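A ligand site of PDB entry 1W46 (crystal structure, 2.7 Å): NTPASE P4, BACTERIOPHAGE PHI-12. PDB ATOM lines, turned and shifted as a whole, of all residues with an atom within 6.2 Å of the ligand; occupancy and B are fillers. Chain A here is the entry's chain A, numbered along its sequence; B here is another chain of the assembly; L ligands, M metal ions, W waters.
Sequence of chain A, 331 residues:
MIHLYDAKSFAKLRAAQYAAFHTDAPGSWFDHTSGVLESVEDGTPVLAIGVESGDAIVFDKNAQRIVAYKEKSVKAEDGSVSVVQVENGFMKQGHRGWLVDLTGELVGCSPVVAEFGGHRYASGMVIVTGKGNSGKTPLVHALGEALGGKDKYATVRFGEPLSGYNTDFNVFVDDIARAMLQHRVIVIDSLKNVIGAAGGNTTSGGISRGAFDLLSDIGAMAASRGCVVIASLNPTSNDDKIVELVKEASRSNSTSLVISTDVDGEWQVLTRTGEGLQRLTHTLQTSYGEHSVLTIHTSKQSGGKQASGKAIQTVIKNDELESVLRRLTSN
N of Thr 137 lies within hydrogen-bond range of O3 of the ligand (3.2 Å). The backbone NH (N) of Lys 136 is in hydrogen-bond range of an oxygen (O3) of the ligand. O of Ser 134 sits at hydrogen-bond distance from O9 of the ligand (3.1 Å). The backbone carbonyl oxygen (O) of Asn 133 lies within hydrogen-bond range of an oxygen (O9) of the ligand, 2.7 Å away. An oxygen (O2) of the ligand sits at hydrogen-bond distance from the backbone NH of Ser 134 (3.0 Å). O4 of the ligand is in salt-bridge range of NH2 of Arg 279 of chain B (2.8 Å). The side-chain hydroxyl (OG) of Ser 292 sits at hydrogen-bond distance from a nitrogen (N2) of the ligand (2.5 Å). O5 of the ligand sits at hydrogen-bond distance from OG1 of Thr 137. The guanidinium group (NH2) of Arg 272 of chain B is in salt-bridge range of an oxygen (O4) of the ligand (3.8 Å). An oxygen (O2) of the ligand sits close to the side-chain amide oxygen (OD1) of Asn 234 (3.3 Å). The side-chain amide nitrogen of Asn 133 sits at hydrogen-bond distance from an oxygen (O9) of the ligand (2.7 Å). The side-chain hydroxyl of Tyr 288 lies within hydrogen-bond range of an oxygen (O8) of the ligand, at 3.3 Å.
OE1 of Glu 160 is in salt-bridge range of NH2 of Arg 272 of chain B. The side-chain amino group (NZ) of Lys 136 is in hydrogen-bond range of the backbone carbonyl oxygen (O) of Lys 131, 3.3 Å away. The side-chain carboxylate (OD1) of Asp 189 sits at hydrogen-bond distance from the side-chain hydroxyl (OG1) of Thr 137. NE of Arg 279 of chain B lies close to ND2 of Asn 133 (3.3 Å). ND2 of Asn 234 lies close to N of Asn 133. OG of Ser 134 sits at hydrogen-bond distance from O of Lys 131 (3.4 Å). The side-chain amino group (NZ) of Lys 136 sits at hydrogen-bond distance from the side-chain amide oxygen (OD1) of Asn 234, at 2.5 Å. OG of Ser 134 is in hydrogen-bond range of NZ of Lys 136 (2.6 Å).
Merely in contact with the ligand: Gly 135, Pro 138, Gly 276 of chain B, Leu 277 of chain B and Gln 278 of chain B. Of the 23 residues printed, 14 come within 4 Å of the ligand. The nearest printed residue that does not touch the ligand is Gly 132 (4.7 Å).
Water W1 lies within hydrogen-bond range of an oxygen (O5) of the ligand (2.6 Å) and the backbone NH of Gly 276 of chain B (3.1 Å). Water W2 lies within hydrogen-bond range of N of Ser 292, N3 of the ligand and O of Gly 289.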
ATOM      1  N   LYS A 131     -21.844 -26.437  24.849  1.00  0.00           N
ATOM      2  CA  LYS A 131     -22.074 -25.761  23.561  1.00  0.00           C
ATOM      3  C   LYS A 131     -21.749 -24.267  23.555  1.00  0.00           C
ATOM      4  O   LYS A 131     -22.518 -23.450  24.055  1.00  0.00           O
ATOM      5  CB  LYS A 131     -23.532 -25.945  23.121  1.00  0.00           C
ATOM      6  CG  LYS A 131     -23.897 -25.176  21.853  1.00  0.00           C
ATOM      7  CD  LYS A 131     -25.401 -25.120  21.610  1.00  0.00           C
ATOM      8  CE  LYS A 131     -26.140 -24.287  22.657  1.00  0.00           C
ATOM      9  NZ  LYS A 131     -26.114 -24.906  24.017  1.00  0.00           N
ATOM     10  N   GLY A 132     -20.609 -23.926  22.957  1.00  0.00           N
ATOM     11  CA  GLY A 132     -20.148 -22.544  22.877  1.00  0.00           C
ATOM     12  C   GLY A 132     -21.178 -21.428  22.813  1.00  0.00           C
ATOM     13  O   GLY A 132     -22.308 -21.617  22.372  1.00  0.00           O
ATOM     14  N   ASN A 133     -20.755 -20.247  23.264  1.00  0.00           N
ATOM     15  CA  ASN A 133     -21.552 -19.020  23.290  1.00  0.00           C
ATOM     16  C   ASN A 133     -22.966 -19.158  23.883  1.00  0.00           C
ATOM     17  O   ASN A 133     -23.895 -18.469  23.459  1.00  0.00           O
ATOM     18  CB  ASN A 133     -21.644 -18.417  21.881  1.00  0.00           C
ATOM     19  CG  ASN A 133     -22.155 -16.971  21.890  1.00  0.00           C
ATOM     20  OD1 ASN A 133     -22.402 -16.378  20.836  1.00  0.00           O
ATOM     21  ND2 ASN A 133     -22.310 -16.402  23.087  1.00  0.00           N
ATOM     22  N   SER A 134     -23.137 -20.048  24.858  1.00  0.00           N
ATOM     23  CA  SER A 134     -24.435 -20.223  25.499  1.00  0.00           C
ATOM     24  C   SER A 134     -24.492 -19.251  26.675  1.00  0.00           C
ATOM     25  O   SER A 134     -23.666 -18.344  26.765  1.00  0.00           O
ATOM     26  CB  SER A 134     -24.609 -21.666  25.988  1.00  0.00           C
ATOM     27  OG  SER A 134     -23.589 -22.031  26.899  1.00  0.00           O
ATOM     28  N   GLY A 135     -25.442 -19.429  27.578  1.00  0.00           N
ATOM     29  CA  GLY A 135     -25.533 -18.512  28.698  1.00  0.00           C
ATOM     30  C   GLY A 135     -24.747 -18.937  29.923  1.00  0.00           C
ATOM     31  O   GLY A 135     -25.317 -19.004  31.018  1.00  0.00           O
ATOM     32  N   LYS A 136     -23.453 -19.190  29.757  1.00  0.00           N
ATOM     33  CA  LYS A 136     -22.629 -19.636  30.885  1.00  0.00           C
ATOM     34  C   LYS A 136     -22.413 -18.588  31.961  1.00  0.00           C
ATOM     35  O   LYS A 136     -22.459 -18.901  33.161  1.00  0.00           O
ATOM     36  CB  LYS A 136     -21.278 -20.167  30.401  1.00  0.00           C
ATOM     37  CG  LYS A 136     -21.408 -21.447  29.617  1.00  0.00           C
ATOM     38  CD  LYS A 136     -20.075 -21.891  29.038  1.00  0.00           C
ATOM     39  CE  LYS A 136     -20.260 -23.006  28.010  1.00  0.00           C
ATOM     40  NZ  LYS A 136     -21.077 -22.564  26.843  1.00  0.00           N
ATOM     41  N   THR A 137     -22.180 -17.344  31.568  1.00  0.00           N
ATOM     42  CA  THR A 137     -21.960 -16.293  32.553  1.00  0.00           C
ATOM     43  C   THR A 137     -23.233 -16.038  33.372  1.00  0.00           C
ATOM     44  O   THR A 137     -23.184 -15.910  34.594  1.00  0.00           O
ATOM     45  CB  THR A 137     -21.473 -15.001  31.883  1.00  0.00           C
ATOM     46  OG1 THR A 137     -20.129 -15.195  31.447  1.00  0.00           O
ATOM     47  CG2 THR A 137     -21.531 -13.829  32.862  1.00  0.00           C
ATOM     48  N   PRO A 138     -24.407 -15.966  32.703  1.00  0.00           N
ATOM     49  CA  PRO A 138     -25.633 -15.734  33.451  1.00  0.00           C
ATOM     50  C   PRO A 138     -25.882 -16.866  34.441  1.00  0.00           C
ATOM     51  O   PRO A 138     -26.372 -16.652  35.541  1.00  0.00           O
ATOM     52  CB  PRO A 138     -26.688 -15.687  32.358  1.00  0.00           C
ATOM     53  CG  PRO A 138     -25.962 -15.110  31.215  1.00  0.00           C
ATOM     54  CD  PRO A 138     -24.657 -15.864  31.255  1.00  0.00           C
ATOM     55  N   GLU A 160     -11.217 -11.711  30.052  1.00  0.00           N
ATOM     56  CA  GLU A 160     -12.308 -11.398  29.127  1.00  0.00           C
ATOM     57  C   GLU A 160     -12.050  -9.955  28.693  1.00  0.00           C
ATOM     58  O   GLU A 160     -11.603  -9.131  29.500  1.00  0.00           O
ATOM     59  CB  GLU A 160     -13.671 -11.511  29.811  1.00  0.00           C
ATOM     60  CG  GLU A 160     -14.153 -12.939  30.102  1.00  0.00           C
ATOM     61  CD  GLU A 160     -14.329 -13.784  28.846  1.00  0.00           C
ATOM     62  OE1 GLU A 160     -14.723 -13.241  27.795  1.00  0.00           O
ATOM     63  OE2 GLU A 160     -14.099 -14.999  28.921  1.00  0.00           O
ATOM     64  N   ASP A 189     -15.268 -15.887  36.689  1.00  0.00           N
ATOM     65  CA  ASP A 189     -15.743 -15.665  35.359  1.00  0.00           C
ATOM     66  C   ASP A 189     -14.642 -15.815  34.355  1.00  0.00           C
ATOM     67  O   ASP A 189     -13.759 -14.961  34.232  1.00  0.00           O
ATOM     68  CB  ASP A 189     -16.394 -14.291  35.207  1.00  0.00           C
ATOM     69  CG  ASP A 189     -17.541 -14.327  34.216  1.00  0.00           C
ATOM     70  OD1 ASP A 189     -17.440 -15.075  33.213  1.00  0.00           O
ATOM     71  OD2 ASP A 189     -18.550 -13.608  34.420  1.00  0.00           O
ATOM     72  N   SER A 232     -16.807 -20.564  34.991  1.00  0.00           N
ATOM     73  CA  SER A 232     -17.292 -20.547  33.621  1.00  0.00           C
ATOM     74  C   SER A 232     -16.191 -21.070  32.724  1.00  0.00           C
ATOM     75  O   SER A 232     -15.031 -20.695  32.874  1.00  0.00           O
ATOM     76  CB  SER A 232     -17.638 -19.109  33.208  1.00  0.00           C
ATOM     77  OG  SER A 232     -17.906 -19.039  31.821  1.00  0.00           O
ATOM     78  N   ASN A 234     -16.190 -21.544  28.735  1.00  0.00           N
ATOM     79  CA  ASN A 234     -16.740 -21.580  27.394  1.00  0.00           C
ATOM     80  C   ASN A 234     -15.634 -22.090  26.483  1.00  0.00           C
ATOM     81  O   ASN A 234     -14.562 -21.490  26.414  1.00  0.00           O
ATOM     82  CB  ASN A 234     -17.182 -20.185  26.955  1.00  0.00           C
ATOM     83  CG  ASN A 234     -18.334 -20.234  25.978  1.00  0.00           C
ATOM     84  OD1 ASN A 234     -19.412 -20.727  26.294  1.00  0.00           O
ATOM     85  ND2 ASN A 234     -18.110 -19.717  24.777  1.00  0.00           N
ATOM     86  N   TYR A 288     -34.582 -15.878  31.567  1.00  0.00           N
ATOM     87  CA  TYR A 288     -34.020 -14.538  31.673  1.00  0.00           C
ATOM     88  C   TYR A 288     -35.056 -13.500  32.080  1.00  0.00           C
ATOM     89  O   TYR A 288     -36.241 -13.618  31.786  1.00  0.00           O
ATOM     90  CB  TYR A 288     -33.407 -14.120  30.320  1.00  0.00           C
ATOM     91  CG  TYR A 288     -32.079 -14.746  30.018  1.00  0.00           C
ATOM     92  CD1 TYR A 288     -30.906 -14.253  30.591  1.00  0.00           C
ATOM     93  CD2 TYR A 288     -31.985 -15.827  29.152  1.00  0.00           C
ATOM     94  CE1 TYR A 288     -29.657 -14.827  30.292  1.00  0.00           C
ATOM     95  CE2 TYR A 288     -30.763 -16.416  28.859  1.00  0.00           C
ATOM     96  CZ  TYR A 288     -29.601 -15.904  29.431  1.00  0.00           C
ATOM     97  OH  TYR A 288     -28.366 -16.465  29.138  1.00  0.00           O
ATOM     98  N   GLY A 289     -34.576 -12.457  32.756  1.00  0.00           N
ATOM     99  CA  GLY A 289     -35.434 -11.375  33.179  1.00  0.00           C
ATOM    100  C   GLY A 289     -34.850 -10.098  32.595  1.00  0.00           C
ATOM    101  O   GLY A 289     -34.276 -10.102  31.497  1.00  0.00           O
ATOM    102  N   HIS A 291     -32.253  -7.030  32.012  1.00  0.00           N
ATOM    103  CA  HIS A 291     -30.803  -6.908  31.982  1.00  0.00           C
ATOM    104  C   HIS A 291     -30.071  -8.248  32.082  1.00  0.00           C
ATOM    105  O   HIS A 291     -29.057  -8.365  32.781  1.00  0.00           O
ATOM    106  CB  HIS A 291     -30.309  -5.984  33.102  1.00  0.00           C
ATOM    107  CG  HIS A 291     -31.070  -4.697  33.177  1.00  0.00           C
ATOM    108  ND1 HIS A 291     -31.358  -3.935  32.062  1.00  0.00           N
ATOM    109  CD2 HIS A 291     -31.604  -4.033  34.232  1.00  0.00           C
ATOM    110  CE1 HIS A 291     -32.046  -2.866  32.436  1.00  0.00           C
ATOM    111  NE2 HIS A 291     -32.201  -2.899  33.739  1.00  0.00           N
ATOM    112  N   SER A 292     -30.608  -9.241  31.400  1.00  0.00           N
ATOM    113  CA  SER A 292     -30.011 -10.575  31.379  1.00  0.00           C
ATOM    114  C   SER A 292     -29.785 -11.260  32.712  1.00  0.00           C
ATOM    115  O   SER A 292     -28.940 -12.149  32.821  1.00  0.00           O
ATOM    116  CB  SER A 292     -28.693 -10.541  30.601  1.00  0.00           C
ATOM    117  OG  SER A 292     -28.942 -10.208  29.251  1.00  0.00           O
ATOM    118  N   ARG B 272     -20.322  -7.610  21.762  1.00  0.00           N
ATOM    119  CA  ARG B 272     -20.570  -8.073  23.119  1.00  0.00           C
ATOM    120  C   ARG B 272     -20.881  -6.766  23.831  1.00  0.00           C
ATOM    121  O   ARG B 272     -20.020  -5.917  23.992  1.00  0.00           O
ATOM    122  CB  ARG B 272     -19.339  -8.745  23.726  1.00  0.00           C
ATOM    123  CG  ARG B 272     -19.075 -10.148  23.174  1.00  0.00           C
ATOM    124  CD  ARG B 272     -17.795 -10.757  23.728  1.00  0.00           C
ATOM    125  NE  ARG B 272     -17.908 -11.133  25.136  1.00  0.00           N
ATOM    126  CZ  ARG B 272     -16.956 -11.788  25.797  1.00  0.00           C
ATOM    127  NH1 ARG B 272     -15.837 -12.127  25.167  1.00  0.00           N
ATOM    128  NH2 ARG B 272     -17.121 -12.098  27.081  1.00  0.00           N
ATOM    129  N   GLY B 274     -21.641  -6.391  26.920  1.00  0.00           N
ATOM    130  CA  GLY B 274     -21.286  -6.382  28.335  1.00  0.00           C
ATOM    131  C   GLY B 274     -21.347  -7.724  29.026  1.00  0.00           C
ATOM    132  O   GLY B 274     -21.882  -8.695  28.497  1.00  0.00           O
ATOM    133  N   GLU B 275     -20.806  -7.785  30.229  1.00  0.00           N
ATOM    134  CA  GLU B 275     -20.765  -8.993  31.026  1.00  0.00           C
ATOM    135  C   GLU B 275     -22.117  -9.692  31.133  1.00  0.00           C
ATOM    136  O   GLU B 275     -23.049  -9.172  31.736  1.00  0.00           O
ATOM    137  CB  GLU B 275     -20.274  -8.661  32.418  1.00  0.00           C
ATOM    138  CG  GLU B 275     -20.153  -9.845  33.342  1.00  0.00           C
ATOM    139  CD  GLU B 275     -19.658  -9.435  34.706  1.00  0.00           C
ATOM    140  OE1 GLU B 275     -20.489  -9.135  35.576  1.00  0.00           O
ATOM    141  OE2 GLU B 275     -18.424  -9.395  34.885  1.00  0.00           O
ATOM    142  N   GLY B 276     -22.196 -10.893  30.554  1.00  0.00           N
ATOM    143  CA  GLY B 276     -23.430 -11.656  30.607  1.00  0.00           C
ATOM    144  C   GLY B 276     -24.605 -11.044  29.862  1.00  0.00           C
ATOM    145  O   GLY B 276     -25.718 -11.588  29.884  1.00  0.00           O
ATOM    146  N   LEU B 277     -24.372  -9.927  29.190  1.00  0.00           N
ATOM    147  CA  LEU B 277     -25.442  -9.273  28.462  1.00  0.00           C
ATOM    148  C   LEU B 277     -25.649  -9.909  27.087  1.00  0.00           C
ATOM    149  O   LEU B 277     -24.891 -10.779  26.673  1.00  0.00           O
ATOM    150  CB  LEU B 277     -25.151  -7.775  28.340  1.00  0.00           C
ATOM    151  CG  LEU B 277     -25.053  -7.063  29.701  1.00  0.00           C
ATOM    152  CD1 LEU B 277     -25.062  -5.569  29.502  1.00  0.00           C
ATOM    153  CD2 LEU B 277     -26.232  -7.459  30.587  1.00  0.00           C
ATOM    154  N   GLN B 278     -26.684  -9.461  26.387  1.00  0.00           N
ATOM    155  CA  GLN B 278     -26.990 -10.001  25.072  1.00  0.00           C
ATOM    156  C   GLN B 278     -25.971  -9.585  24.014  1.00  0.00           C
ATOM    157  O   GLN B 278     -25.443  -8.473  24.040  1.00  0.00           O
ATOM    158  CB  GLN B 278     -28.376  -9.554  24.656  1.00  0.00           C
ATOM    159  CG  GLN B 278     -29.142 -10.580  23.857  1.00  0.00           C
ATOM    160  CD  GLN B 278     -30.636 -10.373  23.931  1.00  0.00           C
ATOM    161  OE1 GLN B 278     -31.412 -11.145  23.379  1.00  0.00           O
ATOM    162  NE2 GLN B 278     -31.056  -9.312  24.630  1.00  0.00           N
ATOM    163  N   ARG B 279     -25.664 -10.492  23.096  1.00  0.00           N
ATOM    164  CA  ARG B 279     -24.719 -10.182  22.033  1.00  0.00           C
ATOM    165  C   ARG B 279     -25.531  -9.669  20.858  1.00  0.00           C
ATOM    166  O   ARG B 279     -26.548 -10.260  20.483  1.00  0.00           O
ATOM    167  CB  ARG B 279     -23.910 -11.425  21.649  1.00  0.00           C
ATOM    168  CG  ARG B 279     -23.154 -12.001  22.833  1.00  0.00           C
ATOM    169  CD  ARG B 279     -22.002 -12.878  22.411  1.00  0.00           C
ATOM    170  NE  ARG B 279     -21.229 -13.331  23.569  1.00  0.00           N
ATOM    171  CZ  ARG B 279     -20.017 -13.861  23.482  1.00  0.00           C
ATOM    172  NH1 ARG B 279     -19.435 -14.027  22.291  1.00  0.00           N
ATOM    173  NH2 ARG B 279     -19.385 -14.254  24.588  1.00  0.00           N
HETATM  174  P1  LIG L   1     -20.934 -17.160  27.320  1.00  0.00           P
HETATM  175  O1  LIG L   1     -19.471 -17.029  27.624  1.00  0.00           O
HETATM  176  O2  LIG L   1     -21.251 -17.967  25.995  1.00  0.00           O
HETATM  177  O3  LIG L   1     -21.605 -17.825  28.450  1.00  0.00           O
HETATM  178  P2  LIG L   1     -21.326 -14.335  27.815  1.00  0.00           P
HETATM  179  O4  LIG L   1     -20.740 -13.396  26.885  1.00  0.00           O
HETATM  180  O5  LIG L   1     -20.487 -14.458  28.974  1.00  0.00           O
HETATM  181  O6  LIG L   1     -21.518 -15.716  27.075  1.00  0.00           O
HETATM  182  O7  LIG L   1     -22.782 -13.996  28.307  1.00  0.00           O
HETATM  183  C1  LIG L   1     -23.759 -13.779  27.354  1.00  0.00           C
HETATM  184  C2  LIG L   1     -24.572 -14.977  26.907  1.00  0.00           C
HETATM  185  O8  LIG L   1     -25.928 -14.940  27.422  1.00  0.00           O
HETATM  186  C3  LIG L   1     -24.621 -14.891  25.459  1.00  0.00           C
HETATM  187  O9  LIG L   1     -24.455 -16.141  24.786  1.00  0.00           O
HETATM  188  C4  LIG L   1     -25.939 -14.208  25.181  1.00  0.00           C
HETATM  189  O10 LIG L   1     -26.300 -14.403  23.825  1.00  0.00           O
HETATM  190  C5  LIG L   1     -26.849 -14.815  26.305  1.00  0.00           C
HETATM  191  N1  LIG L   1     -28.002 -13.909  26.791  1.00  0.00           N
HETATM  192  C6  LIG L   1     -27.857 -12.823  27.566  1.00  0.00           C
HETATM  193  N2  LIG L   1     -29.049 -12.251  27.802  1.00  0.00           N
HETATM  194  C7  LIG L   1     -29.955 -12.925  27.208  1.00  0.00           C
HETATM  195  C8  LIG L   1     -31.333 -12.828  27.095  1.00  0.00           C
HETATM  196  N3  LIG L   1     -31.970 -11.828  27.697  1.00  0.00           N
HETATM  197  N4  LIG L   1     -32.035 -13.729  26.367  1.00  0.00           N
HETATM  198  C9  LIG L   1     -31.425 -14.757  25.732  1.00  0.00           C
HETATM  199  N5  LIG L   1     -30.070 -14.885  25.826  1.00  0.00           N
HETATM  200  C10 LIG L   1     -29.310 -14.008  26.539  1.00  0.00           C
HETATM  201 MG    MG M   1     -18.285 -16.539  30.066  1.00  0.00          MG
HETATM  202  O   HOH W   1     -19.576 -12.162  29.614  1.00  0.00           O
HETATM  203  O   HOH W   2     -32.430  -9.148  29.055  1.00  0.00           O
